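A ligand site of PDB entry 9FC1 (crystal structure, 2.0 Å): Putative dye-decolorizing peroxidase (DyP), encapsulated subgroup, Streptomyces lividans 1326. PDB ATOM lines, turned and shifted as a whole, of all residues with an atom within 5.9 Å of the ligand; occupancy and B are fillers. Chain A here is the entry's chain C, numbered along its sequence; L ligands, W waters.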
ATOM      1  N   ASP A 146     -16.769 -30.360  32.005  1.00  0.00           N
ATOM      2  CA  ASP A 146     -15.945 -30.796  33.116  1.00  0.00           C
ATOM      3  C   ASP A 146     -16.400 -30.031  34.371  1.00  0.00           C
ATOM      4  O   ASP A 146     -17.360 -29.273  34.331  1.00  0.00           O
ATOM      5  CB  ASP A 146     -14.456 -30.722  32.755  1.00  0.00           C
ATOM      6  CG  ASP A 146     -13.951 -29.338  32.392  1.00  0.00           C
ATOM      7  OD1 ASP A 146     -14.604 -28.297  32.880  1.00  0.00           O
ATOM      8  OD2 ASP A 146     -12.955 -29.311  31.561  1.00  0.00           O
ATOM      9  N   LEU A 148     -15.143 -27.472  35.757  1.00  0.00           N
ATOM     10  CA  LEU A 148     -15.016 -26.043  35.553  1.00  0.00           C
ATOM     11  C   LEU A 148     -16.174 -25.443  34.748  1.00  0.00           C
ATOM     12  O   LEU A 148     -16.273 -24.215  34.636  1.00  0.00           O
ATOM     13  CB  LEU A 148     -13.665 -25.726  34.901  1.00  0.00           C
ATOM     14  CG  LEU A 148     -12.421 -26.191  35.690  1.00  0.00           C
ATOM     15  CD1 LEU A 148     -11.174 -25.714  35.003  1.00  0.00           C
ATOM     16  CD2 LEU A 148     -12.411 -25.678  37.128  1.00  0.00           C
ATOM     17  N   PHE A 150     -16.776 -26.010  31.500  1.00  0.00           N
ATOM     18  CA  PHE A 150     -16.428 -25.903  30.107  1.00  0.00           C
ATOM     19  C   PHE A 150     -16.579 -27.282  29.444  1.00  0.00           C
ATOM     20  O   PHE A 150     -16.236 -28.323  30.029  1.00  0.00           O
ATOM     21  CB  PHE A 150     -15.018 -25.341  29.896  1.00  0.00           C
ATOM     22  CG  PHE A 150     -14.930 -23.842  30.088  1.00  0.00           C
ATOM     23  CD1 PHE A 150     -15.128 -23.276  31.346  1.00  0.00           C
ATOM     24  CD2 PHE A 150     -14.714 -22.999  29.008  1.00  0.00           C
ATOM     25  CE1 PHE A 150     -15.082 -21.887  31.525  1.00  0.00           C
ATOM     26  CE2 PHE A 150     -14.669 -21.610  29.187  1.00  0.00           C
ATOM     27  CZ  PHE A 150     -14.847 -21.054  30.452  1.00  0.00           C
ATOM     28  N   VAL A 151     -16.970 -27.242  28.170  1.00  0.00           N
ATOM     29  CA  VAL A 151     -16.964 -28.430  27.337  1.00  0.00           C
ATOM     30  C   VAL A 151     -15.524 -28.913  27.211  1.00  0.00           C
ATOM     31  O   VAL A 151     -14.599 -28.120  27.027  1.00  0.00           O
ATOM     32  CB  VAL A 151     -17.576 -28.117  25.955  1.00  0.00           C
ATOM     33  CG1 VAL A 151     -17.556 -29.362  25.041  1.00  0.00           C
ATOM     34  CG2 VAL A 151     -18.993 -27.572  26.094  1.00  0.00           C
ATOM     35  N   ASP A 152     -15.361 -30.237  27.341  1.00  0.00           N
ATOM     36  CA  ASP A 152     -14.064 -30.854  27.442  1.00  0.00           C
ATOM     37  C   ASP A 152     -13.992 -32.011  26.435  1.00  0.00           C
ATOM     38  O   ASP A 152     -14.740 -32.979  26.571  1.00  0.00           O
ATOM     39  CB  ASP A 152     -13.885 -31.326  28.895  1.00  0.00           C
ATOM     40  CG  ASP A 152     -12.477 -31.695  29.288  1.00  0.00           C
ATOM     41  OD1 ASP A 152     -11.827 -32.402  28.452  1.00  0.00           O
ATOM     42  OD2 ASP A 152     -12.036 -31.262  30.416  1.00  0.00           O
ATOM     43  N   GLY A 153     -13.111 -31.876  25.425  1.00  0.00           N
ATOM     44  CA  GLY A 153     -12.955 -32.894  24.368  1.00  0.00           C
ATOM     45  C   GLY A 153     -13.059 -32.361  22.943  1.00  0.00           C
ATOM     46  O   GLY A 153     -12.709 -33.047  21.997  1.00  0.00           O
ATOM     47  N   THR A 154     -13.501 -31.102  22.803  1.00  0.00           N
ATOM     48  CA  THR A 154     -13.892 -30.533  21.537  1.00  0.00           C
ATOM     49  C   THR A 154     -12.838 -30.692  20.449  1.00  0.00           C
ATOM     50  O   THR A 154     -13.195 -31.128  19.364  1.00  0.00           O
ATOM     51  CB  THR A 154     -14.163 -29.031  21.691  1.00  0.00           C
ATOM     52  OG1 THR A 154     -15.036 -28.906  22.830  1.00  0.00           O
ATOM     53  CG2 THR A 154     -14.807 -28.456  20.449  1.00  0.00           C
ATOM     54  N   GLU A 155     -11.558 -30.339  20.700  1.00  0.00           N
ATOM     55  CA  GLU A 155     -10.536 -30.365  19.650  1.00  0.00           C
ATOM     56  C   GLU A 155      -9.801 -31.712  19.566  1.00  0.00           C
ATOM     57  O   GLU A 155      -8.795 -31.798  18.888  1.00  0.00           O
ATOM     58  CB  GLU A 155      -9.572 -29.171  19.786  1.00  0.00           C
ATOM     59  CG  GLU A 155     -10.221 -27.828  19.377  1.00  0.00           C
ATOM     60  CD  GLU A 155     -10.670 -27.805  17.931  1.00  0.00           C
ATOM     61  OE1 GLU A 155      -9.852 -27.968  17.115  1.00  0.00           O
ATOM     62  OE2 GLU A 155     -11.842 -27.679  17.620  1.00  0.00           O
ATOM     63  N   ASN A 156     -10.294 -32.766  20.215  1.00  0.00           N
ATOM     64  CA  ASN A 156      -9.685 -34.079  19.981  1.00  0.00           C
ATOM     65  C   ASN A 156      -9.720 -34.436  18.487  1.00  0.00           C
ATOM     66  O   ASN A 156     -10.704 -34.188  17.788  1.00  0.00           O
ATOM     67  CB  ASN A 156     -10.398 -35.203  20.736  1.00  0.00           C
ATOM     68  CG  ASN A 156      -9.890 -35.430  22.141  1.00  0.00           C
ATOM     69  OD1 ASN A 156      -8.695 -35.228  22.444  1.00  0.00           O
ATOM     70  ND2 ASN A 156     -10.799 -35.828  23.031  1.00  0.00           N
ATOM     71  N   GLN A 184      -2.814 -37.874  35.153  1.00  0.00           N
ATOM     72  CA  GLN A 184      -2.646 -36.945  36.254  1.00  0.00           C
ATOM     73  C   GLN A 184      -4.013 -36.698  36.877  1.00  0.00           C
ATOM     74  O   GLN A 184      -4.969 -36.269  36.222  1.00  0.00           O
ATOM     75  CB  GLN A 184      -2.086 -35.571  35.837  1.00  0.00           C
ATOM     76  CG  GLN A 184      -0.715 -35.525  35.190  1.00  0.00           C
ATOM     77  CD  GLN A 184      -0.353 -34.098  34.850  1.00  0.00           C
ATOM     78  OE1 GLN A 184      -0.990 -33.476  34.002  1.00  0.00           O
ATOM     79  NE2 GLN A 184       0.572 -33.508  35.616  1.00  0.00           N
ATOM     80  N   TYR A 186      -6.180 -34.282  39.004  1.00  0.00           N
ATOM     81  CA  TYR A 186      -6.218 -32.873  39.396  1.00  0.00           C
ATOM     82  C   TYR A 186      -7.415 -32.601  40.307  1.00  0.00           C
ATOM     83  O   TYR A 186      -8.515 -33.136  40.080  1.00  0.00           O
ATOM     84  CB  TYR A 186      -6.361 -31.938  38.183  1.00  0.00           C
ATOM     85  CG  TYR A 186      -5.143 -31.747  37.307  1.00  0.00           C
ATOM     86  CD1 TYR A 186      -4.861 -32.586  36.248  1.00  0.00           C
ATOM     87  CD2 TYR A 186      -4.280 -30.690  37.530  1.00  0.00           C
ATOM     88  CE1 TYR A 186      -3.768 -32.374  35.417  1.00  0.00           C
ATOM     89  CE2 TYR A 186      -3.136 -30.502  36.761  1.00  0.00           C
ATOM     90  CZ  TYR A 186      -2.902 -31.315  35.668  1.00  0.00           C
ATOM     91  OH  TYR A 186      -1.765 -31.161  34.896  1.00  0.00           O
ATOM     92  N   HIS A 188      -9.545 -29.306  42.032  1.00  0.00           N
ATOM     93  CA  HIS A 188      -9.774 -27.919  41.665  1.00  0.00           C
ATOM     94  C   HIS A 188     -10.148 -27.092  42.899  1.00  0.00           C
ATOM     95  O   HIS A 188     -10.740 -27.608  43.836  1.00  0.00           O
ATOM     96  CB  HIS A 188     -10.899 -27.852  40.635  1.00  0.00           C
ATOM     97  CG  HIS A 188     -10.549 -28.459  39.330  1.00  0.00           C
ATOM     98  ND1 HIS A 188      -9.549 -27.944  38.526  1.00  0.00           N
ATOM     99  CD2 HIS A 188     -11.078 -29.527  38.678  1.00  0.00           C
ATOM    100  CE1 HIS A 188      -9.479 -28.694  37.406  1.00  0.00           C
ATOM    101  NE2 HIS A 188     -10.402 -29.639  37.469  1.00  0.00           N
ATOM    102  N   ILE A 205      -9.301 -20.249  29.901  1.00  0.00           N
ATOM    103  CA  ILE A 205      -9.399 -21.459  29.094  1.00  0.00           C
ATOM    104  C   ILE A 205      -8.996 -21.152  27.647  1.00  0.00           C
ATOM    105  O   ILE A 205      -8.245 -21.899  27.041  1.00  0.00           O
ATOM    106  CB  ILE A 205     -10.833 -22.047  29.182  1.00  0.00           C
ATOM    107  CG1 ILE A 205     -11.252 -22.428  30.597  1.00  0.00           C
ATOM    108  CG2 ILE A 205     -10.977 -23.241  28.257  1.00  0.00           C
ATOM    109  CD1 ILE A 205     -10.351 -23.523  31.284  1.00  0.00           C
ATOM    110  N   ARG A 207     -11.679 -20.301  25.301  1.00  0.00           N
ATOM    111  CA  ARG A 207     -12.878 -20.560  24.519  1.00  0.00           C
ATOM    112  C   ARG A 207     -14.049 -19.927  25.269  1.00  0.00           C
ATOM    113  O   ARG A 207     -13.917 -19.691  26.460  1.00  0.00           O
ATOM    114  CB  ARG A 207     -13.134 -22.060  24.414  1.00  0.00           C
ATOM    115  CG  ARG A 207     -11.941 -22.890  23.919  1.00  0.00           C
ATOM    116  CD  ARG A 207     -12.233 -24.392  23.746  1.00  0.00           C
ATOM    117  NE  ARG A 207     -13.148 -24.648  22.644  1.00  0.00           N
ATOM    118  CZ  ARG A 207     -12.797 -24.718  21.355  1.00  0.00           C
ATOM    119  NH1 ARG A 207     -11.547 -24.881  21.006  1.00  0.00           N
ATOM    120  NH2 ARG A 207     -13.707 -24.693  20.424  1.00  0.00           N
ATOM    121  N   ASP A 212     -18.763 -22.661  23.424  1.00  0.00           N
ATOM    122  CA  ASP A 212     -17.552 -23.424  23.148  1.00  0.00           C
ATOM    123  C   ASP A 212     -16.851 -22.961  21.885  1.00  0.00           C
ATOM    124  O   ASP A 212     -16.158 -23.737  21.252  1.00  0.00           O
ATOM    125  CB  ASP A 212     -17.840 -24.928  23.025  1.00  0.00           C
ATOM    126  CG  ASP A 212     -16.607 -25.799  23.201  1.00  0.00           C
ATOM    127  OD1 ASP A 212     -15.594 -25.326  23.793  1.00  0.00           O
ATOM    128  OD2 ASP A 212     -16.705 -26.953  22.796  1.00  0.00           O
ATOM    129  N   GLU A 214     -13.934 -20.954  20.046  1.00  0.00           N
ATOM    130  CA  GLU A 214     -12.589 -20.503  20.366  1.00  0.00           C
ATOM    131  C   GLU A 214     -12.478 -18.975  20.239  1.00  0.00           C
ATOM    132  O   GLU A 214     -13.038 -18.411  19.325  1.00  0.00           O
ATOM    133  CB  GLU A 214     -11.624 -21.224  19.402  1.00  0.00           C
ATOM    134  CG  GLU A 214     -10.176 -20.954  19.639  1.00  0.00           C
ATOM    135  CD  GLU A 214      -9.240 -21.916  18.917  1.00  0.00           C
ATOM    136  OE1 GLU A 214      -9.774 -22.926  18.323  1.00  0.00           O
ATOM    137  OE2 GLU A 214      -8.017 -21.702  19.016  1.00  0.00           O
ATOM    138  N   HIS A 225      -5.146 -21.801  28.534  1.00  0.00           N
ATOM    139  CA  HIS A 225      -4.922 -23.235  28.392  1.00  0.00           C
ATOM    140  C   HIS A 225      -4.795 -23.662  26.918  1.00  0.00           C
ATOM    141  O   HIS A 225      -3.908 -24.417  26.521  1.00  0.00           O
ATOM    142  CB  HIS A 225      -6.053 -23.976  29.110  1.00  0.00           C
ATOM    143  CG  HIS A 225      -5.876 -25.436  29.096  1.00  0.00           C
ATOM    144  ND1 HIS A 225      -4.748 -26.040  29.640  1.00  0.00           N
ATOM    145  CD2 HIS A 225      -6.694 -26.441  28.650  1.00  0.00           C
ATOM    146  CE1 HIS A 225      -4.864 -27.373  29.462  1.00  0.00           C
ATOM    147  NE2 HIS A 225      -6.057 -27.634  28.908  1.00  0.00           N
ATOM    148  N   VAL A 226      -5.715 -23.139  26.085  1.00  0.00           N
ATOM    149  CA  VAL A 226      -5.690 -23.476  24.661  1.00  0.00           C
ATOM    150  C   VAL A 226      -4.409 -22.977  23.969  1.00  0.00           C
ATOM    151  O   VAL A 226      -3.890 -23.663  23.099  1.00  0.00           O
ATOM    152  CB  VAL A 226      -6.955 -22.944  23.974  1.00  0.00           C
ATOM    153  CG1 VAL A 226      -6.801 -22.850  22.479  1.00  0.00           C
ATOM    154  CG2 VAL A 226      -8.114 -23.812  24.373  1.00  0.00           C
ATOM    155  N   THR A 229      -1.376 -25.230  25.021  1.00  0.00           N
ATOM    156  CA  THR A 229      -1.432 -26.649  24.639  1.00  0.00           C
ATOM    157  C   THR A 229      -1.540 -26.849  23.135  1.00  0.00           C
ATOM    158  O   THR A 229      -1.610 -27.999  22.684  1.00  0.00           O
ATOM    159  CB  THR A 229      -2.514 -27.415  25.406  1.00  0.00           C
ATOM    160  OG1 THR A 229      -3.802 -26.847  25.152  1.00  0.00           O
ATOM    161  CG2 THR A 229      -2.188 -27.396  26.887  1.00  0.00           C
ATOM    162  N   SER A 230      -1.543 -25.731  22.383  1.00  0.00           N
ATOM    163  CA  SER A 230      -1.413 -25.723  20.921  1.00  0.00           C
ATOM    164  C   SER A 230       0.047 -25.682  20.545  1.00  0.00           C
ATOM    165  O   SER A 230       0.726 -24.740  20.918  1.00  0.00           O
ATOM    166  CB  SER A 230      -2.150 -24.551  20.331  1.00  0.00           C
ATOM    167  OG  SER A 230      -3.555 -24.664  20.681  1.00  0.00           O
ATOM    168  N   ILE A 241      -2.790 -34.867  20.578  1.00  0.00           N
ATOM    169  CA  ILE A 241      -2.994 -36.003  21.465  1.00  0.00           C
ATOM    170  C   ILE A 241      -4.492 -36.282  21.548  1.00  0.00           C
ATOM    171  O   ILE A 241      -5.280 -35.494  21.125  1.00  0.00           O
ATOM    172  CB  ILE A 241      -2.413 -35.737  22.854  1.00  0.00           C
ATOM    173  CG1 ILE A 241      -3.180 -34.656  23.619  1.00  0.00           C
ATOM    174  CG2 ILE A 241      -0.928 -35.470  22.773  1.00  0.00           C
ATOM    175  CD1 ILE A 241      -2.710 -34.520  25.089  1.00  0.00           C
ATOM    176  N   ARG A 243      -7.406 -37.086  24.296  1.00  0.00           N
ATOM    177  CA  ARG A 243      -7.702 -36.983  25.705  1.00  0.00           C
ATOM    178  C   ARG A 243      -9.084 -37.585  25.990  1.00  0.00           C
ATOM    179  O   ARG A 243      -9.904 -37.585  25.109  1.00  0.00           O
ATOM    180  CB  ARG A 243      -7.729 -35.535  26.142  1.00  0.00           C
ATOM    181  CG  ARG A 243      -6.397 -34.841  26.052  1.00  0.00           C
ATOM    182  CD  ARG A 243      -6.550 -33.328  26.122  1.00  0.00           C
ATOM    183  NE  ARG A 243      -7.206 -32.833  24.918  1.00  0.00           N
ATOM    184  CZ  ARG A 243      -8.372 -32.143  24.897  1.00  0.00           C
ATOM    185  NH1 ARG A 243      -8.989 -31.799  26.025  1.00  0.00           N
ATOM    186  NH2 ARG A 243      -8.903 -31.799  23.711  1.00  0.00           N
ATOM    187  N   ASN A 245     -10.674 -36.957  29.407  1.00  0.00           N
ATOM    188  CA  ASN A 245     -10.781 -36.439  30.762  1.00  0.00           C
ATOM    189  C   ASN A 245     -12.144 -36.762  31.408  1.00  0.00           C
ATOM    190  O   ASN A 245     -13.209 -36.649  30.789  1.00  0.00           O
ATOM    191  CB  ASN A 245     -10.559 -34.926  30.797  1.00  0.00           C
ATOM    192  CG  ASN A 245      -9.191 -34.522  30.292  1.00  0.00           C
ATOM    193  OD1 ASN A 245      -8.292 -35.342  30.087  1.00  0.00           O
ATOM    194  ND2 ASN A 245      -9.084 -33.222  30.010  1.00  0.00           N
ATOM    195  N   THR A 258     -10.719 -33.323  38.077  1.00  0.00           N
ATOM    196  CA  THR A 258     -10.588 -33.772  36.727  1.00  0.00           C
ATOM    197  C   THR A 258      -9.490 -34.835  36.664  1.00  0.00           C
ATOM    198  O   THR A 258      -8.355 -34.560  37.072  1.00  0.00           O
ATOM    199  CB  THR A 258     -10.203 -32.633  35.779  1.00  0.00           C
ATOM    200  OG1 THR A 258     -11.191 -31.623  35.808  1.00  0.00           O
ATOM    201  CG2 THR A 258     -10.082 -33.105  34.346  1.00  0.00           C
ATOM    202  N   PHE A 260      -7.175 -36.486  34.272  1.00  0.00           N
ATOM    203  CA  PHE A 260      -6.548 -36.295  32.980  1.00  0.00           C
ATOM    204  C   PHE A 260      -5.936 -37.590  32.480  1.00  0.00           C
ATOM    205  O   PHE A 260      -5.158 -38.213  33.173  1.00  0.00           O
ATOM    206  CB  PHE A 260      -5.482 -35.180  33.035  1.00  0.00           C
ATOM    207  CG  PHE A 260      -4.666 -35.071  31.770  1.00  0.00           C
ATOM    208  CD1 PHE A 260      -5.163 -34.426  30.670  1.00  0.00           C
ATOM    209  CD2 PHE A 260      -3.459 -35.711  31.667  1.00  0.00           C
ATOM    210  CE1 PHE A 260      -4.435 -34.436  29.483  1.00  0.00           C
ATOM    211  CE2 PHE A 260      -2.725 -35.698  30.498  1.00  0.00           C
ATOM    212  CZ  PHE A 260      -3.245 -35.115  29.386  1.00  0.00           C
ATOM    213  N   THR A 270       3.161 -35.096  24.510  1.00  0.00           N
ATOM    214  CA  THR A 270       2.489 -34.826  25.779  1.00  0.00           C
ATOM    215  C   THR A 270       3.428 -34.072  26.727  1.00  0.00           C
ATOM    216  O   THR A 270       3.011 -33.159  27.413  1.00  0.00           O
ATOM    217  CB  THR A 270       1.983 -36.120  26.455  1.00  0.00           C
ATOM    218  OG1 THR A 270       1.330 -36.904  25.455  1.00  0.00           O
ATOM    219  CG2 THR A 270       1.069 -35.790  27.612  1.00  0.00           C
ATOM    220  N   MET A 273       3.750 -30.375  25.874  1.00  0.00           N
ATOM    221  CA  MET A 273       2.586 -29.677  26.410  1.00  0.00           C
ATOM    222  C   MET A 273       2.714 -29.424  27.906  1.00  0.00           C
ATOM    223  O   MET A 273       2.463 -28.312  28.392  1.00  0.00           O
ATOM    224  CB  MET A 273       1.310 -30.419  26.121  1.00  0.00           C
ATOM    225  CG  MET A 273       0.937 -30.426  24.671  1.00  0.00           C
ATOM    226  SD  MET A 273      -0.434 -31.527  24.321  1.00  0.00           S
ATOM    227  CE  MET A 273      -0.534 -31.371  22.536  1.00  0.00           C
ATOM    228  N   LEU A 274       3.115 -30.440  28.668  1.00  0.00           N
ATOM    229  CA  LEU A 274       3.290 -30.295  30.122  1.00  0.00           C
ATOM    230  C   LEU A 274       4.381 -29.255  30.439  1.00  0.00           C
ATOM    231  O   LEU A 274       4.212 -28.473  31.373  1.00  0.00           O
ATOM    232  CB  LEU A 274       3.646 -31.648  30.730  1.00  0.00           C
ATOM    233  CG  LEU A 274       2.446 -32.628  30.858  1.00  0.00           C
ATOM    234  CD1 LEU A 274       2.864 -34.072  31.170  1.00  0.00           C
ATOM    235  CD2 LEU A 274       1.468 -32.127  31.954  1.00  0.00           C
ATOM    236  N   MET A 277       2.918 -25.823  30.017  1.00  0.00           N
ATOM    237  CA  MET A 277       1.966 -25.491  31.070  1.00  0.00           C
ATOM    238  C   MET A 277       2.652 -25.131  32.390  1.00  0.00           C
ATOM    239  O   MET A 277       2.206 -24.206  33.070  1.00  0.00           O
ATOM    240  CB  MET A 277       0.997 -26.644  31.324  1.00  0.00           C
ATOM    241  CG  MET A 277      -0.001 -26.940  30.184  1.00  0.00           C
ATOM    242  SD  MET A 277      -0.966 -28.469  30.498  1.00  0.00           S
ATOM    243  CE  MET A 277      -1.787 -27.998  32.004  1.00  0.00           C
ATOM    244  N   PHE A 278       3.607 -25.962  32.830  1.00  0.00           N
ATOM    245  CA  PHE A 278       4.216 -25.841  34.146  1.00  0.00           C
ATOM    246  C   PHE A 278       5.461 -24.901  34.167  1.00  0.00           C
ATOM    247  O   PHE A 278       5.694 -24.228  35.175  1.00  0.00           O
ATOM    248  CB  PHE A 278       4.554 -27.224  34.716  1.00  0.00           C
ATOM    249  CG  PHE A 278       3.349 -27.998  35.224  1.00  0.00           C
ATOM    250  CD1 PHE A 278       2.557 -28.711  34.358  1.00  0.00           C
ATOM    251  CD2 PHE A 278       3.010 -27.978  36.538  1.00  0.00           C
ATOM    252  CE1 PHE A 278       1.446 -29.396  34.790  1.00  0.00           C
ATOM    253  CE2 PHE A 278       1.893 -28.646  36.984  1.00  0.00           C
ATOM    254  CZ  PHE A 278       1.119 -29.364  36.103  1.00  0.00           C
ATOM    255  N   ILE A 289      -4.805 -22.274  34.028  1.00  0.00           N
ATOM    256  CA  ILE A 289      -5.686 -23.297  34.581  1.00  0.00           C
ATOM    257  C   ILE A 289      -5.060 -23.872  35.861  1.00  0.00           C
ATOM    258  O   ILE A 289      -5.778 -24.323  36.725  1.00  0.00           O
ATOM    259  CB  ILE A 289      -6.037 -24.397  33.522  1.00  0.00           C
ATOM    260  CG1 ILE A 289      -7.406 -25.028  33.773  1.00  0.00           C
ATOM    261  CG2 ILE A 289      -4.951 -25.466  33.455  1.00  0.00           C
ATOM    262  CD1 ILE A 289      -7.814 -26.064  32.734  1.00  0.00           C
ATOM    263  N   SER A 293      -6.147 -25.548  39.787  1.00  0.00           N
ATOM    264  CA  SER A 293      -6.009 -26.969  39.558  1.00  0.00           C
ATOM    265  C   SER A 293      -4.653 -27.444  40.081  1.00  0.00           C
ATOM    266  O   SER A 293      -3.632 -26.995  39.596  1.00  0.00           O
ATOM    267  CB  SER A 293      -6.094 -27.318  38.053  1.00  0.00           C
ATOM    268  OG  SER A 293      -7.217 -26.766  37.443  1.00  0.00           O
HETATM  269  C1  LIG L   1      -8.104 -28.421  25.604  1.00  0.00           C
HETATM  270  C2  LIG L   1      -9.624 -28.830  30.186  1.00  0.00           C
HETATM  271  C3  LIG L   1      -5.274 -30.541  31.488  1.00  0.00           C
HETATM  272  C4  LIG L   1      -4.095 -30.766  26.839  1.00  0.00           C
HETATM  273  C5  LIG L   1      -8.876 -28.255  26.758  1.00  0.00           C
HETATM  274  C6  LIG L   1     -10.157 -27.625  26.847  1.00  0.00           C
HETATM  275  C7  LIG L   1     -10.586 -27.789  28.125  1.00  0.00           C
HETATM  276  C8  LIG L   1      -9.638 -28.492  28.832  1.00  0.00           C
HETATM  277  C9  LIG L   1     -11.820 -27.276  28.751  1.00  0.00           C
HETATM  278  C10 LIG L   1     -10.858 -26.911  25.710  1.00  0.00           C
HETATM  279  C11 LIG L   1     -11.813 -27.791  24.891  1.00  0.00           C
HETATM  280  C12 LIG L   1     -11.075 -28.967  24.253  1.00  0.00           C
HETATM  281  O1  LIG L   1     -10.592 -28.850  23.146  1.00  0.00           O
HETATM  282  O2  LIG L   1     -11.100 -30.064  24.841  1.00  0.00           O
HETATM  283  C13 LIG L   1      -8.553 -29.343  30.976  1.00  0.00           C
HETATM  284  C14 LIG L   1      -8.577 -29.545  32.434  1.00  0.00           C
HETATM  285  C15 LIG L   1      -7.361 -30.050  32.795  1.00  0.00           C
HETATM  286  C16 LIG L   1      -6.575 -30.107  31.550  1.00  0.00           C
HETATM  287  C17 LIG L   1      -9.843 -29.231  33.283  1.00  0.00           C
HETATM  288  C18 LIG L   1      -6.741 -30.340  34.081  1.00  0.00           C
HETATM  289  C19 LIG L   1      -7.034 -29.597  35.102  1.00  0.00           C
HETATM  290  C20 LIG L   1      -4.543 -30.763  30.351  1.00  0.00           C
HETATM  291  C21 LIG L   1      -3.237 -31.278  30.290  1.00  0.00           C
HETATM  292  C22 LIG L   1      -2.843 -31.318  28.951  1.00  0.00           C
HETATM  293  C23 LIG L   1      -4.001 -30.854  28.218  1.00  0.00           C
HETATM  294  C24 LIG L   1      -2.496 -31.662  31.525  1.00  0.00           C
HETATM  295  C25 LIG L   1      -1.626 -31.859  28.301  1.00  0.00           C
HETATM  296  C26 LIG L   1      -0.761 -32.501  28.973  1.00  0.00           C
HETATM  297  C27 LIG L   1      -5.098 -30.155  26.183  1.00  0.00           C
HETATM  298  C28 LIG L   1      -5.121 -30.039  24.717  1.00  0.00           C
HETATM  299  C29 LIG L   1      -6.212 -29.357  24.340  1.00  0.00           C
HETATM  300  C30 LIG L   1      -6.872 -29.069  25.585  1.00  0.00           C
HETATM  301  C31 LIG L   1      -4.091 -30.538  23.780  1.00  0.00           C
HETATM  302  C32 LIG L   1      -6.683 -28.991  22.946  1.00  0.00           C
HETATM  303  C33 LIG L   1      -6.147 -27.607  22.573  1.00  0.00           C
HETATM  304  C34 LIG L   1      -6.368 -27.233  21.091  1.00  0.00           C
HETATM  305  O3  LIG L   1      -7.415 -26.575  20.812  1.00  0.00           O
HETATM  306  O4  LIG L   1      -5.515 -27.624  20.238  1.00  0.00           O
HETATM  307  N1  LIG L   1      -8.603 -28.786  27.980  1.00  0.00           N
HETATM  308  N2  LIG L   1      -7.340 -29.668  30.547  1.00  0.00           N
HETATM  309  N3  LIG L   1      -4.957 -30.477  29.103  1.00  0.00           N
HETATM  310  N4  LIG L   1      -6.179 -29.587  26.660  1.00  0.00           N
HETATM  311 FE1  LIG L   1      -6.816 -29.575  28.532  1.00  0.00          FE
HETATM  312  O   HOH W   1      -9.592 -26.433  22.500  1.00  0.00           O
HETATM  313  O   HOH W   2      -3.520 -29.317  20.693  1.00  0.00           O
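An iron atom (FE1) of the ligand is bound by a ring nitrogen (NE2) of His 225 (2.1 Å). N of Gly 153 lies within hydrogen-bond range of O2 of the ligand (2.8 Å). NH1 of Arg 243 is in salt-bridge range of O2 of the ligand (3.0 Å). O1 of the ligand is in hydrogen-bond range of N of Glu 155. N of Thr 154 lies within hydrogen-bond range of O2 of the ligand.
The backbone carbonyl oxygen (O) of His 225 is in hydrogen-bond range of the side-chain hydroxyl (OG1) of Thr 229 (2.8 Å). The backbone NH of His 225 lies within hydrogen-bond range of the backbone carbonyl oxygen of Ile 205, at 3.4 Å. The side-chain carboxylate (OD2) of Asp 146 lies close to the side-chain carboxylate (OD2) of Asp 152 (2.4 Å). ND1 of His 188 is in hydrogen-bond range of OG of Ser 293, 2.8 Å away. N of Tyr 186 lies within hydrogen-bond range of O of Thr 258. The backbone NH (N) of Leu 148 sits at hydrogen-bond distance from the side-chain carboxylate (OD1) of Asp 146, at 3.0 Å. The backbone carbonyl oxygen (O) of Ile 289 sits at hydrogen-bond distance from the side-chain hydroxyl (OG) of Ser 293, 2.9 Å away. The side-chain hydroxyl (OG) of Ser 230 sits at hydrogen-bond distance from the backbone carbonyl oxygen (O) of Val 226 (2.6 Å).
OD2 of Asp 146 touches C17 of the ligand, 3.6 Å away. Phe 150 touches the ligand (CB to C9, 3.9 Å). Val 151 touches the ligand (O to C9, 3.4 Å). Asp 152 touches the ligand (OD2 to C2, 3.4 Å). OE1 of Gln 184 touches C24 of the ligand, 3.4 Å away. Tyr 186 touches the ligand. His 188 touches the ligand (CE1 to C19, 3.5 Å). Arg 207 touches the ligand (CD to C10, 3.5 Å). Thr 229 touches the ligand. OG of Ser 230 touches O4 of the ligand, 3.6 Å away. Asn 245 touches the ligand (ND2 to N2, 3.995 Å). Thr 258 touches the ligand. CE1 of Phe 260 touches C21 of the ligand, 3.5 Å away. Met 273 touches the ligand (SD to C31, 3.8 Å). Leu 274 touches the ligand (CG to C26, 3.7 Å). SD of Met 277 touches C21 of the ligand, at 3.6 Å. CD1 of Ile 289 touches C14 of the ligand (3.6 Å). Ser 293 touches the ligand. Hydrophobic or aromatic side chains within 4 Å of the ligand: Phe 150, Tyr 186, His 188, His 225, Phe 260, Met 273, Leu 274, Met 277 and Ile 289. Within 4 Å of the ligand: Asp 146, Phe 150, Val 151, Asp 152, Gly 153, Thr 154, Glu 155, Gln 184, Tyr 186, His 188, Arg 207, His 225, Thr 229, Ser 230, Arg 243, Asn 245, Thr 258, Phe 260, Met 273, Leu 274, Met 277, Ile 289 and Ser 293. Along chain A the residues within 4 Å of the ligand span positions 146 to 293. The nearest printed residue that does not touch the ligand is Thr 270 (4.002 Å).
Water W2 lies within hydrogen-bond range of an oxygen (O4) of the ligand and the backbone carbonyl oxygen of Thr 229. Water W1 lies within hydrogen-bond range of O1 of the ligand and NH1 of Arg 207.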
